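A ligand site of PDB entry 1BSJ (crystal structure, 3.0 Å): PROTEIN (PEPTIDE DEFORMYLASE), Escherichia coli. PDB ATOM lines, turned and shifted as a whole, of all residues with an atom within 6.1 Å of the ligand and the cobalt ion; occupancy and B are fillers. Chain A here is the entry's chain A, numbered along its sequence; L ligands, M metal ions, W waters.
The side-chain carboxylate (OE1) of Glu 88 sits at hydrogen-bond distance from a ring nitrogen (ND1) of His 132 (2.8 Å). The backbone NH of Ser 92 sits close to the side-chain sulfur of Cys 90. The side-chain amide oxygen (OE1) of Gln 50 lies close to the side-chain carboxylate (OE1) of Glu 133, at 3.5 Å. The side-chain carboxylate (OE1) of Glu 133 lies close to the backbone NH (N) of Leu 46 (3.4 Å). The backbone NH of Ala 47 sits at hydrogen-bond distance from the side-chain carboxylate of Glu 133 (3.0 Å). The backbone carbonyl oxygen (O) of Ile 44 is in hydrogen-bond range of the side-chain sulfur (SG) of Cys 129, at 3.7 Å. The side-chain amide nitrogen (NE2) of Gln 50 lies within hydrogen-bond range of the side-chain hydroxyl (OG) of Ser 92 (3.4 Å). OE1 of Gln 50 sits at hydrogen-bond distance from N of Ala 47, at 2.9 Å.
The backbone NH of Leu 91 lies within hydrogen-bond range of an oxygen (O3) of the ligand (2.6 Å). O1 of the ligand lies close to OE2 of Glu 133. The backbone NH of Ile 44 lies within hydrogen-bond range of an oxygen (O4) of the ligand, 2.9 Å away. The backbone NH of Gly 89 lies within hydrogen-bond range of an oxygen (O5) of the ligand. The backbone carbonyl oxygen (O) of Gly 89 is in hydrogen-bond range of a nitrogen (N1) of the ligand. An oxygen (O3) of the ligand sits at hydrogen-bond distance from the side-chain amide nitrogen (NE2) of Gln 50.
Residues that only touch the cobalt ion: Gln 50. Four residues have an atom within 4 Å of the cobalt ion: Gln 50, Cys 90, His 132 and His 136. The nearest printed residue that does not touch the cobalt ion is Glu 133 (4.4 Å).
NE2 of His 132 is bound to the cobalt ion (2.1 Å). The cobalt ion is bound by a ring nitrogen (NE2) of His 136 (2.1 Å). O1 of the ligand is bound to the cobalt ion (2.2 Å). The cobalt ion is bound by SG of Cys 90, 2.4 Å away.
O of Gly 45 lies close to O2 of the ligand (3.1 Å). Merely in contact with the ligand: Glu 41, Glu 42, Gly 43, Ile 86, Glu 87, Glu 88, Arg 97 and Cys 129.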
ATOM      1  N   GLU A  41      14.853  21.833 -25.764  1.00  0.00           N
ATOM      2  CA  GLU A  41      15.871  20.883 -25.319  1.00  0.00           C
ATOM      3  C   GLU A  41      16.910  20.607 -26.396  1.00  0.00           C
ATOM      4  O   GLU A  41      17.791  19.798 -26.201  1.00  0.00           O
ATOM      5  CB  GLU A  41      15.227  19.566 -24.946  1.00  0.00           C
ATOM      6  CG  GLU A  41      14.006  19.687 -24.056  1.00  0.00           C
ATOM      7  CD  GLU A  41      14.350  19.766 -22.590  1.00  0.00           C
ATOM      8  OE1 GLU A  41      14.913  20.796 -22.183  1.00  0.00           O
ATOM      9  OE2 GLU A  41      14.038  18.807 -21.835  1.00  0.00           O
ATOM     10  N   GLU A  42      16.776  21.237 -27.561  1.00  0.00           N
ATOM     11  CA  GLU A  42      17.721  21.050 -28.653  1.00  0.00           C
ATOM     12  C   GLU A  42      17.714  19.620 -29.239  1.00  0.00           C
ATOM     13  O   GLU A  42      18.750  19.111 -29.694  1.00  0.00           O
ATOM     14  CB  GLU A  42      19.140  21.450 -28.242  1.00  0.00           C
ATOM     15  CG  GLU A  42      19.272  22.903 -27.829  1.00  0.00           C
ATOM     16  CD  GLU A  42      20.715  23.347 -27.673  1.00  0.00           C
ATOM     17  OE1 GLU A  42      21.298  23.113 -26.594  1.00  0.00           O
ATOM     18  OE2 GLU A  42      21.282  23.924 -28.629  1.00  0.00           O
ATOM     19  N   GLY A  43      16.542  18.991 -29.237  1.00  0.00           N
ATOM     20  CA  GLY A  43      16.403  17.650 -29.770  1.00  0.00           C
ATOM     21  C   GLY A  43      16.008  17.732 -31.222  1.00  0.00           C
ATOM     22  O   GLY A  43      15.560  18.791 -31.652  1.00  0.00           O
ATOM     23  N   ILE A  44      16.190  16.642 -31.978  1.00  0.00           N
ATOM     24  CA  ILE A  44      15.822  16.646 -33.387  1.00  0.00           C
ATOM     25  C   ILE A  44      14.518  15.903 -33.652  1.00  0.00           C
ATOM     26  O   ILE A  44      14.066  15.809 -34.788  1.00  0.00           O
ATOM     27  CB  ILE A  44      16.952  16.089 -34.296  1.00  0.00           C
ATOM     28  CG1 ILE A  44      17.148  14.587 -34.065  1.00  0.00           C
ATOM     29  CG2 ILE A  44      18.258  16.798 -34.001  1.00  0.00           C
ATOM     30  CD1 ILE A  44      18.350  13.979 -34.843  1.00  0.00           C
ATOM     31  N   GLY A  45      13.897  15.402 -32.590  1.00  0.00           N
ATOM     32  CA  GLY A  45      12.650  14.684 -32.686  1.00  0.00           C
ATOM     33  C   GLY A  45      12.061  14.518 -31.295  1.00  0.00           C
ATOM     34  O   GLY A  45      12.768  14.727 -30.316  1.00  0.00           O
ATOM     35  N   LEU A  46      10.778  14.173 -31.198  1.00  0.00           N
ATOM     36  CA  LEU A  46      10.125  13.996 -29.893  1.00  0.00           C
ATOM     37  C   LEU A  46       8.820  13.216 -30.058  1.00  0.00           C
ATOM     38  O   LEU A  46       7.929  13.622 -30.829  1.00  0.00           O
ATOM     39  CB  LEU A  46       9.792  15.342 -29.235  1.00  0.00           C
ATOM     40  CG  LEU A  46       9.240  15.287 -27.803  1.00  0.00           C
ATOM     41  CD1 LEU A  46      10.369  15.004 -26.827  1.00  0.00           C
ATOM     42  CD2 LEU A  46       8.571  16.574 -27.430  1.00  0.00           C
ATOM     43  N   ALA A  47       8.718  12.102 -29.354  1.00  0.00           N
ATOM     44  CA  ALA A  47       7.539  11.272 -29.400  1.00  0.00           C
ATOM     45  C   ALA A  47       6.651  11.649 -28.220  1.00  0.00           C
ATOM     46  O   ALA A  47       7.155  11.973 -27.154  1.00  0.00           O
ATOM     47  CB  ALA A  47       7.926   9.829 -29.329  1.00  0.00           C
ATOM     48  N   GLN A  50       7.129  10.434 -24.519  1.00  0.00           N
ATOM     49  CA  GLN A  50       8.185  11.016 -23.693  1.00  0.00           C
ATOM     50  C   GLN A  50       7.658  12.121 -22.795  1.00  0.00           C
ATOM     51  O   GLN A  50       8.259  12.433 -21.770  1.00  0.00           O
ATOM     52  CB  GLN A  50       9.292  11.589 -24.569  1.00  0.00           C
ATOM     53  CG  GLN A  50      10.056  10.567 -25.377  1.00  0.00           C
ATOM     54  CD  GLN A  50      11.073  11.232 -26.292  1.00  0.00           C
ATOM     55  OE1 GLN A  50      10.792  11.478 -27.459  1.00  0.00           O
ATOM     56  NE2 GLN A  50      12.235  11.546 -25.763  1.00  0.00           N
ATOM     57  N   ILE A  86      24.185   5.461 -36.037  1.00  0.00           N
ATOM     58  CA  ILE A  86      24.844   6.645 -35.511  1.00  0.00           C
ATOM     59  C   ILE A  86      24.815   6.587 -33.977  1.00  0.00           C
ATOM     60  O   ILE A  86      24.146   5.727 -33.390  1.00  0.00           O
ATOM     61  CB  ILE A  86      24.144   7.956 -35.953  1.00  0.00           C
ATOM     62  CG1 ILE A  86      22.751   8.067 -35.332  1.00  0.00           C
ATOM     63  CG2 ILE A  86      24.021   8.040 -37.454  1.00  0.00           C
ATOM     64  CD1 ILE A  86      22.153   9.425 -35.526  1.00  0.00           C
ATOM     65  N   GLU A  87      25.579   7.462 -33.325  1.00  0.00           N
ATOM     66  CA  GLU A  87      25.605   7.522 -31.881  1.00  0.00           C
ATOM     67  C   GLU A  87      24.358   8.266 -31.442  1.00  0.00           C
ATOM     68  O   GLU A  87      24.370   9.491 -31.279  1.00  0.00           O
ATOM     69  CB  GLU A  87      26.820   8.294 -31.391  1.00  0.00           C
ATOM     70  CG  GLU A  87      28.098   7.900 -32.059  1.00  0.00           C
ATOM     71  CD  GLU A  87      28.959   7.023 -31.185  1.00  0.00           C
ATOM     72  OE1 GLU A  87      28.467   5.943 -30.796  1.00  0.00           O
ATOM     73  OE2 GLU A  87      30.107   7.417 -30.896  1.00  0.00           O
ATOM     74  N   GLU A  88      23.280   7.527 -31.253  1.00  0.00           N
ATOM     75  CA  GLU A  88      22.019   8.141 -30.844  1.00  0.00           C
ATOM     76  C   GLU A  88      22.011   8.536 -29.393  1.00  0.00           C
ATOM     77  O   GLU A  88      22.738   7.978 -28.569  1.00  0.00           O
ATOM     78  CB  GLU A  88      20.861   7.186 -31.117  1.00  0.00           C
ATOM     79  CG  GLU A  88      20.649   6.913 -32.568  1.00  0.00           C
ATOM     80  CD  GLU A  88      19.509   5.971 -32.837  1.00  0.00           C
ATOM     81  OE1 GLU A  88      18.496   6.045 -32.105  1.00  0.00           O
ATOM     82  OE2 GLU A  88      19.621   5.173 -33.789  1.00  0.00           O
ATOM     83  N   GLY A  89      21.181   9.518 -29.100  1.00  0.00           N
ATOM     84  CA  GLY A  89      21.014  10.017 -27.752  1.00  0.00           C
ATOM     85  C   GLY A  89      19.523  10.136 -27.593  1.00  0.00           C
ATOM     86  O   GLY A  89      18.784   9.852 -28.529  1.00  0.00           O
ATOM     87  N   CYS A  90      19.062  10.491 -26.402  1.00  0.00           N
ATOM     88  CA  CYS A  90      17.641  10.583 -26.160  1.00  0.00           C
ATOM     89  C   CYS A  90      17.437  11.507 -24.945  1.00  0.00           C
ATOM     90  O   CYS A  90      18.207  11.454 -23.992  1.00  0.00           O
ATOM     91  CB  CYS A  90      17.127   9.167 -25.904  1.00  0.00           C
ATOM     92  SG  CYS A  90      15.332   9.114 -25.658  1.00  0.00           S
ATOM     93  N   LEU A  91      16.412  12.335 -24.967  1.00  0.00           N
ATOM     94  CA  LEU A  91      16.171  13.232 -23.852  1.00  0.00           C
ATOM     95  C   LEU A  91      15.767  12.437 -22.603  1.00  0.00           C
ATOM     96  O   LEU A  91      16.008  12.887 -21.481  1.00  0.00           O
ATOM     97  CB  LEU A  91      15.115  14.273 -24.233  1.00  0.00           C
ATOM     98  CG  LEU A  91      15.628  15.296 -25.266  1.00  0.00           C
ATOM     99  CD1 LEU A  91      14.469  16.076 -25.855  1.00  0.00           C
ATOM    100  CD2 LEU A  91      16.670  16.237 -24.651  1.00  0.00           C
ATOM    101  N   SER A  92      15.224  11.231 -22.831  1.00  0.00           N
ATOM    102  CA  SER A  92      14.770  10.344 -21.760  1.00  0.00           C
ATOM    103  C   SER A  92      15.878   9.480 -21.169  1.00  0.00           C
ATOM    104  O   SER A  92      15.658   8.732 -20.211  1.00  0.00           O
ATOM    105  CB  SER A  92      13.622   9.460 -22.245  1.00  0.00           C
ATOM    106  OG  SER A  92      12.500  10.240 -22.618  1.00  0.00           O
ATOM    107  N   ARG A  97      24.980   7.718 -25.010  1.00  0.00           N
ATOM    108  CA  ARG A  97      24.928   7.640 -26.456  1.00  0.00           C
ATOM    109  C   ARG A  97      25.415   6.277 -26.877  1.00  0.00           C
ATOM    110  O   ARG A  97      26.387   5.775 -26.350  1.00  0.00           O
ATOM    111  CB  ARG A  97      25.848   8.692 -27.083  1.00  0.00           C
ATOM    112  CG  ARG A  97      25.527  10.126 -26.726  1.00  0.00           C
ATOM    113  CD  ARG A  97      25.011  10.895 -27.908  1.00  0.00           C
ATOM    114  NE  ARG A  97      24.560  12.221 -27.502  1.00  0.00           N
ATOM    115  CZ  ARG A  97      24.590  13.292 -28.295  1.00  0.00           C
ATOM    116  NH1 ARG A  97      25.044  13.204 -29.543  1.00  0.00           N
ATOM    117  NH2 ARG A  97      24.200  14.489 -27.816  1.00  0.00           N
ATOM    118  N   LEU A 125      19.769  10.808 -41.899  1.00  0.00           N
ATOM    119  CA  LEU A 125      19.395  11.103 -40.539  1.00  0.00           C
ATOM    120  C   LEU A 125      17.889  11.085 -40.303  1.00  0.00           C
ATOM    121  O   LEU A 125      17.416  10.567 -39.277  1.00  0.00           O
ATOM    122  CB  LEU A 125      19.965  12.454 -40.128  1.00  0.00           C
ATOM    123  CG  LEU A 125      19.864  12.814 -38.656  1.00  0.00           C
ATOM    124  CD1 LEU A 125      20.825  11.967 -37.867  1.00  0.00           C
ATOM    125  CD2 LEU A 125      20.178  14.293 -38.453  1.00  0.00           C
ATOM    126  N   ILE A 128      16.644   7.616 -39.743  1.00  0.00           N
ATOM    127  CA  ILE A 128      17.014   7.128 -38.430  1.00  0.00           C
ATOM    128  C   ILE A 128      16.122   7.702 -37.337  1.00  0.00           C
ATOM    129  O   ILE A 128      15.576   6.958 -36.517  1.00  0.00           O
ATOM    130  CB  ILE A 128      18.488   7.460 -38.108  1.00  0.00           C
ATOM    131  CG1 ILE A 128      19.399   6.790 -39.136  1.00  0.00           C
ATOM    132  CG2 ILE A 128      18.837   6.996 -36.705  1.00  0.00           C
ATOM    133  CD1 ILE A 128      20.841   6.974 -38.857  1.00  0.00           C
ATOM    134  N   CYS A 129      15.942   9.021 -37.374  1.00  0.00           N
ATOM    135  CA  CYS A 129      15.122   9.731 -36.404  1.00  0.00           C
ATOM    136  C   CYS A 129      13.736   9.123 -36.354  1.00  0.00           C
ATOM    137  O   CYS A 129      13.257   8.785 -35.281  1.00  0.00           O
ATOM    138  CB  CYS A 129      15.054  11.196 -36.775  1.00  0.00           C
ATOM    139  SG  CYS A 129      14.326  12.241 -35.545  1.00  0.00           S
ATOM    140  N   HIS A 132      13.669   5.927 -34.533  1.00  0.00           N
ATOM    141  CA  HIS A 132      13.858   6.184 -33.108  1.00  0.00           C
ATOM    142  C   HIS A 132      12.546   6.622 -32.487  1.00  0.00           C
ATOM    143  O   HIS A 132      12.118   6.071 -31.478  1.00  0.00           O
ATOM    144  CB  HIS A 132      14.929   7.252 -32.910  1.00  0.00           C
ATOM    145  CG  HIS A 132      15.214   7.580 -31.468  1.00  0.00           C
ATOM    146  ND1 HIS A 132      16.415   7.391 -30.853  1.00  0.00           N
ATOM    147  CD2 HIS A 132      14.432   8.210 -30.544  1.00  0.00           C
ATOM    148  CE1 HIS A 132      16.365   7.913 -29.620  1.00  0.00           C
ATOM    149  NE2 HIS A 132      15.170   8.417 -29.415  1.00  0.00           N
ATOM    150  N   GLU A 133      11.947   7.646 -33.068  1.00  0.00           N
ATOM    151  CA  GLU A 133      10.690   8.202 -32.581  1.00  0.00           C
ATOM    152  C   GLU A 133       9.530   7.232 -32.594  1.00  0.00           C
ATOM    153  O   GLU A 133       8.688   7.277 -31.710  1.00  0.00           O
ATOM    154  CB  GLU A 133      10.323   9.454 -33.371  1.00  0.00           C
ATOM    155  CG  GLU A 133      11.338  10.561 -33.227  1.00  0.00           C
ATOM    156  CD  GLU A 133      11.746  10.819 -31.793  1.00  0.00           C
ATOM    157  OE1 GLU A 133      10.891  10.744 -30.875  1.00  0.00           O
ATOM    158  OE2 GLU A 133      12.928  11.107 -31.570  1.00  0.00           O
ATOM    159  N   HIS A 136       9.672   4.803 -29.748  1.00  0.00           N
ATOM    160  CA  HIS A 136       9.155   5.463 -28.556  1.00  0.00           C
ATOM    161  C   HIS A 136       7.649   5.253 -28.408  1.00  0.00           C
ATOM    162  O   HIS A 136       7.151   5.218 -27.286  1.00  0.00           O
ATOM    163  CB  HIS A 136       9.402   6.972 -28.622  1.00  0.00           C
ATOM    164  CG  HIS A 136      10.653   7.402 -27.941  1.00  0.00           C
ATOM    165  ND1 HIS A 136      11.023   7.004 -26.678  1.00  0.00           N
ATOM    166  CD2 HIS A 136      11.655   8.202 -28.382  1.00  0.00           C
ATOM    167  CE1 HIS A 136      12.210   7.541 -26.412  1.00  0.00           C
ATOM    168  NE2 HIS A 136      12.617   8.276 -27.421  1.00  0.00           N
ATOM    169  N   LEU A 141      12.905   1.834 -26.239  1.00  0.00           N
ATOM    170  CA  LEU A 141      13.958   2.855 -26.105  1.00  0.00           C
ATOM    171  C   LEU A 141      15.180   2.345 -26.846  1.00  0.00           C
ATOM    172  O   LEU A 141      15.310   1.129 -27.015  1.00  0.00           O
ATOM    173  CB  LEU A 141      14.302   3.052 -24.636  1.00  0.00           C
ATOM    174  CG  LEU A 141      13.171   3.719 -23.834  1.00  0.00           C
ATOM    175  CD1 LEU A 141      13.400   3.518 -22.360  1.00  0.00           C
ATOM    176  CD2 LEU A 141      13.139   5.182 -24.159  1.00  0.00           C
ATOM    177  N   PHE A 142      16.086   3.232 -27.233  1.00  0.00           N
ATOM    178  CA  PHE A 142      17.266   2.767 -27.964  1.00  0.00           C
ATOM    179  C   PHE A 142      18.198   1.817 -27.209  1.00  0.00           C
ATOM    180  O   PHE A 142      18.961   1.094 -27.829  1.00  0.00           O
ATOM    181  CB  PHE A 142      18.053   3.937 -28.576  1.00  0.00           C
ATOM    182  CG  PHE A 142      19.001   4.625 -27.626  1.00  0.00           C
ATOM    183  CD1 PHE A 142      20.206   4.024 -27.262  1.00  0.00           C
ATOM    184  CD2 PHE A 142      18.696   5.856 -27.109  1.00  0.00           C
ATOM    185  CE1 PHE A 142      21.091   4.677 -26.394  1.00  0.00           C
ATOM    186  CE2 PHE A 142      19.567   6.513 -26.244  1.00  0.00           C
ATOM    187  CZ  PHE A 142      20.767   5.920 -25.884  1.00  0.00           C
HETATM  188  O1  LIG L   1      13.570  11.193 -28.804  1.00  0.00           O
HETATM  189  P1  LIG L   1      14.179  12.619 -28.493  1.00  0.00           P
HETATM  190  O2  LIG L   1      15.236  12.886 -29.793  1.00  0.00           O
HETATM  191  O3  LIG L   1      15.052  12.408 -27.234  1.00  0.00           O
HETATM  192  C1  LIG L   1      16.382  12.098 -29.886  1.00  0.00           C
HETATM  193  C2  LIG L   1      17.388  13.258 -30.013  1.00  0.00           C
HETATM  194  C3  LIG L   1      16.086  11.307 -31.184  1.00  0.00           C
HETATM  195  C4  LIG L   1      16.856  11.662 -32.417  1.00  0.00           C
HETATM  196  C5  LIG L   1      17.399  10.515 -33.291  1.00  0.00           C
HETATM  197  C6  LIG L   1      18.414   9.856 -32.390  1.00  0.00           C
HETATM  198  O4  LIG L   1      17.032  14.363 -30.399  1.00  0.00           O
HETATM  199  N1  LIG L   1      18.684  12.964 -29.650  1.00  0.00           N
HETATM  200  C7  LIG L   1      19.814  13.902 -29.801  1.00  0.00           C
HETATM  201  C8  LIG L   1      20.477  14.224 -28.450  1.00  0.00           C
HETATM  202  C9  LIG L   1      19.430  14.851 -27.535  1.00  0.00           C
HETATM  203  C10 LIG L   1      19.804  14.705 -26.104  1.00  0.00           C
HETATM  204  C11 LIG L   1      19.223  16.329 -27.558  1.00  0.00           C
HETATM  205  C12 LIG L   1      20.753  13.215 -30.797  1.00  0.00           C
HETATM  206  N2  LIG L   1      21.162  14.012 -32.024  1.00  0.00           N
HETATM  207  O5  LIG L   1      21.193  12.079 -30.658  1.00  0.00           O
HETATM  208  C13 LIG L   1      22.004  13.704 -32.956  1.00  0.00           C
HETATM  209  C14 LIG L   1      22.806  12.550 -32.865  1.00  0.00           C
HETATM  210  C15 LIG L   1      23.724  12.290 -33.894  1.00  0.00           C
HETATM  211  C16 LIG L   1      23.774  13.176 -35.019  1.00  0.00           C
HETATM  212  C17 LIG L   1      22.953  14.331 -35.133  1.00  0.00           C
HETATM  213  C18 LIG L   1      22.062  14.604 -34.067  1.00  0.00           C
HETATM  214  N3  LIG L   1      24.688  12.890 -36.067  1.00  0.00           N
HETATM  215  O6  LIG L   1      24.639  13.708 -37.131  1.00  0.00           O
HETATM  216  O7  LIG L   1      25.556  11.862 -36.013  1.00  0.00           O
HETATM  217 CO    CO M   1      14.329   9.422 -27.795  1.00  0.00          CO
HETATM  218  O   HOH W   1      15.176   6.313 -27.197  1.00  0.00           O
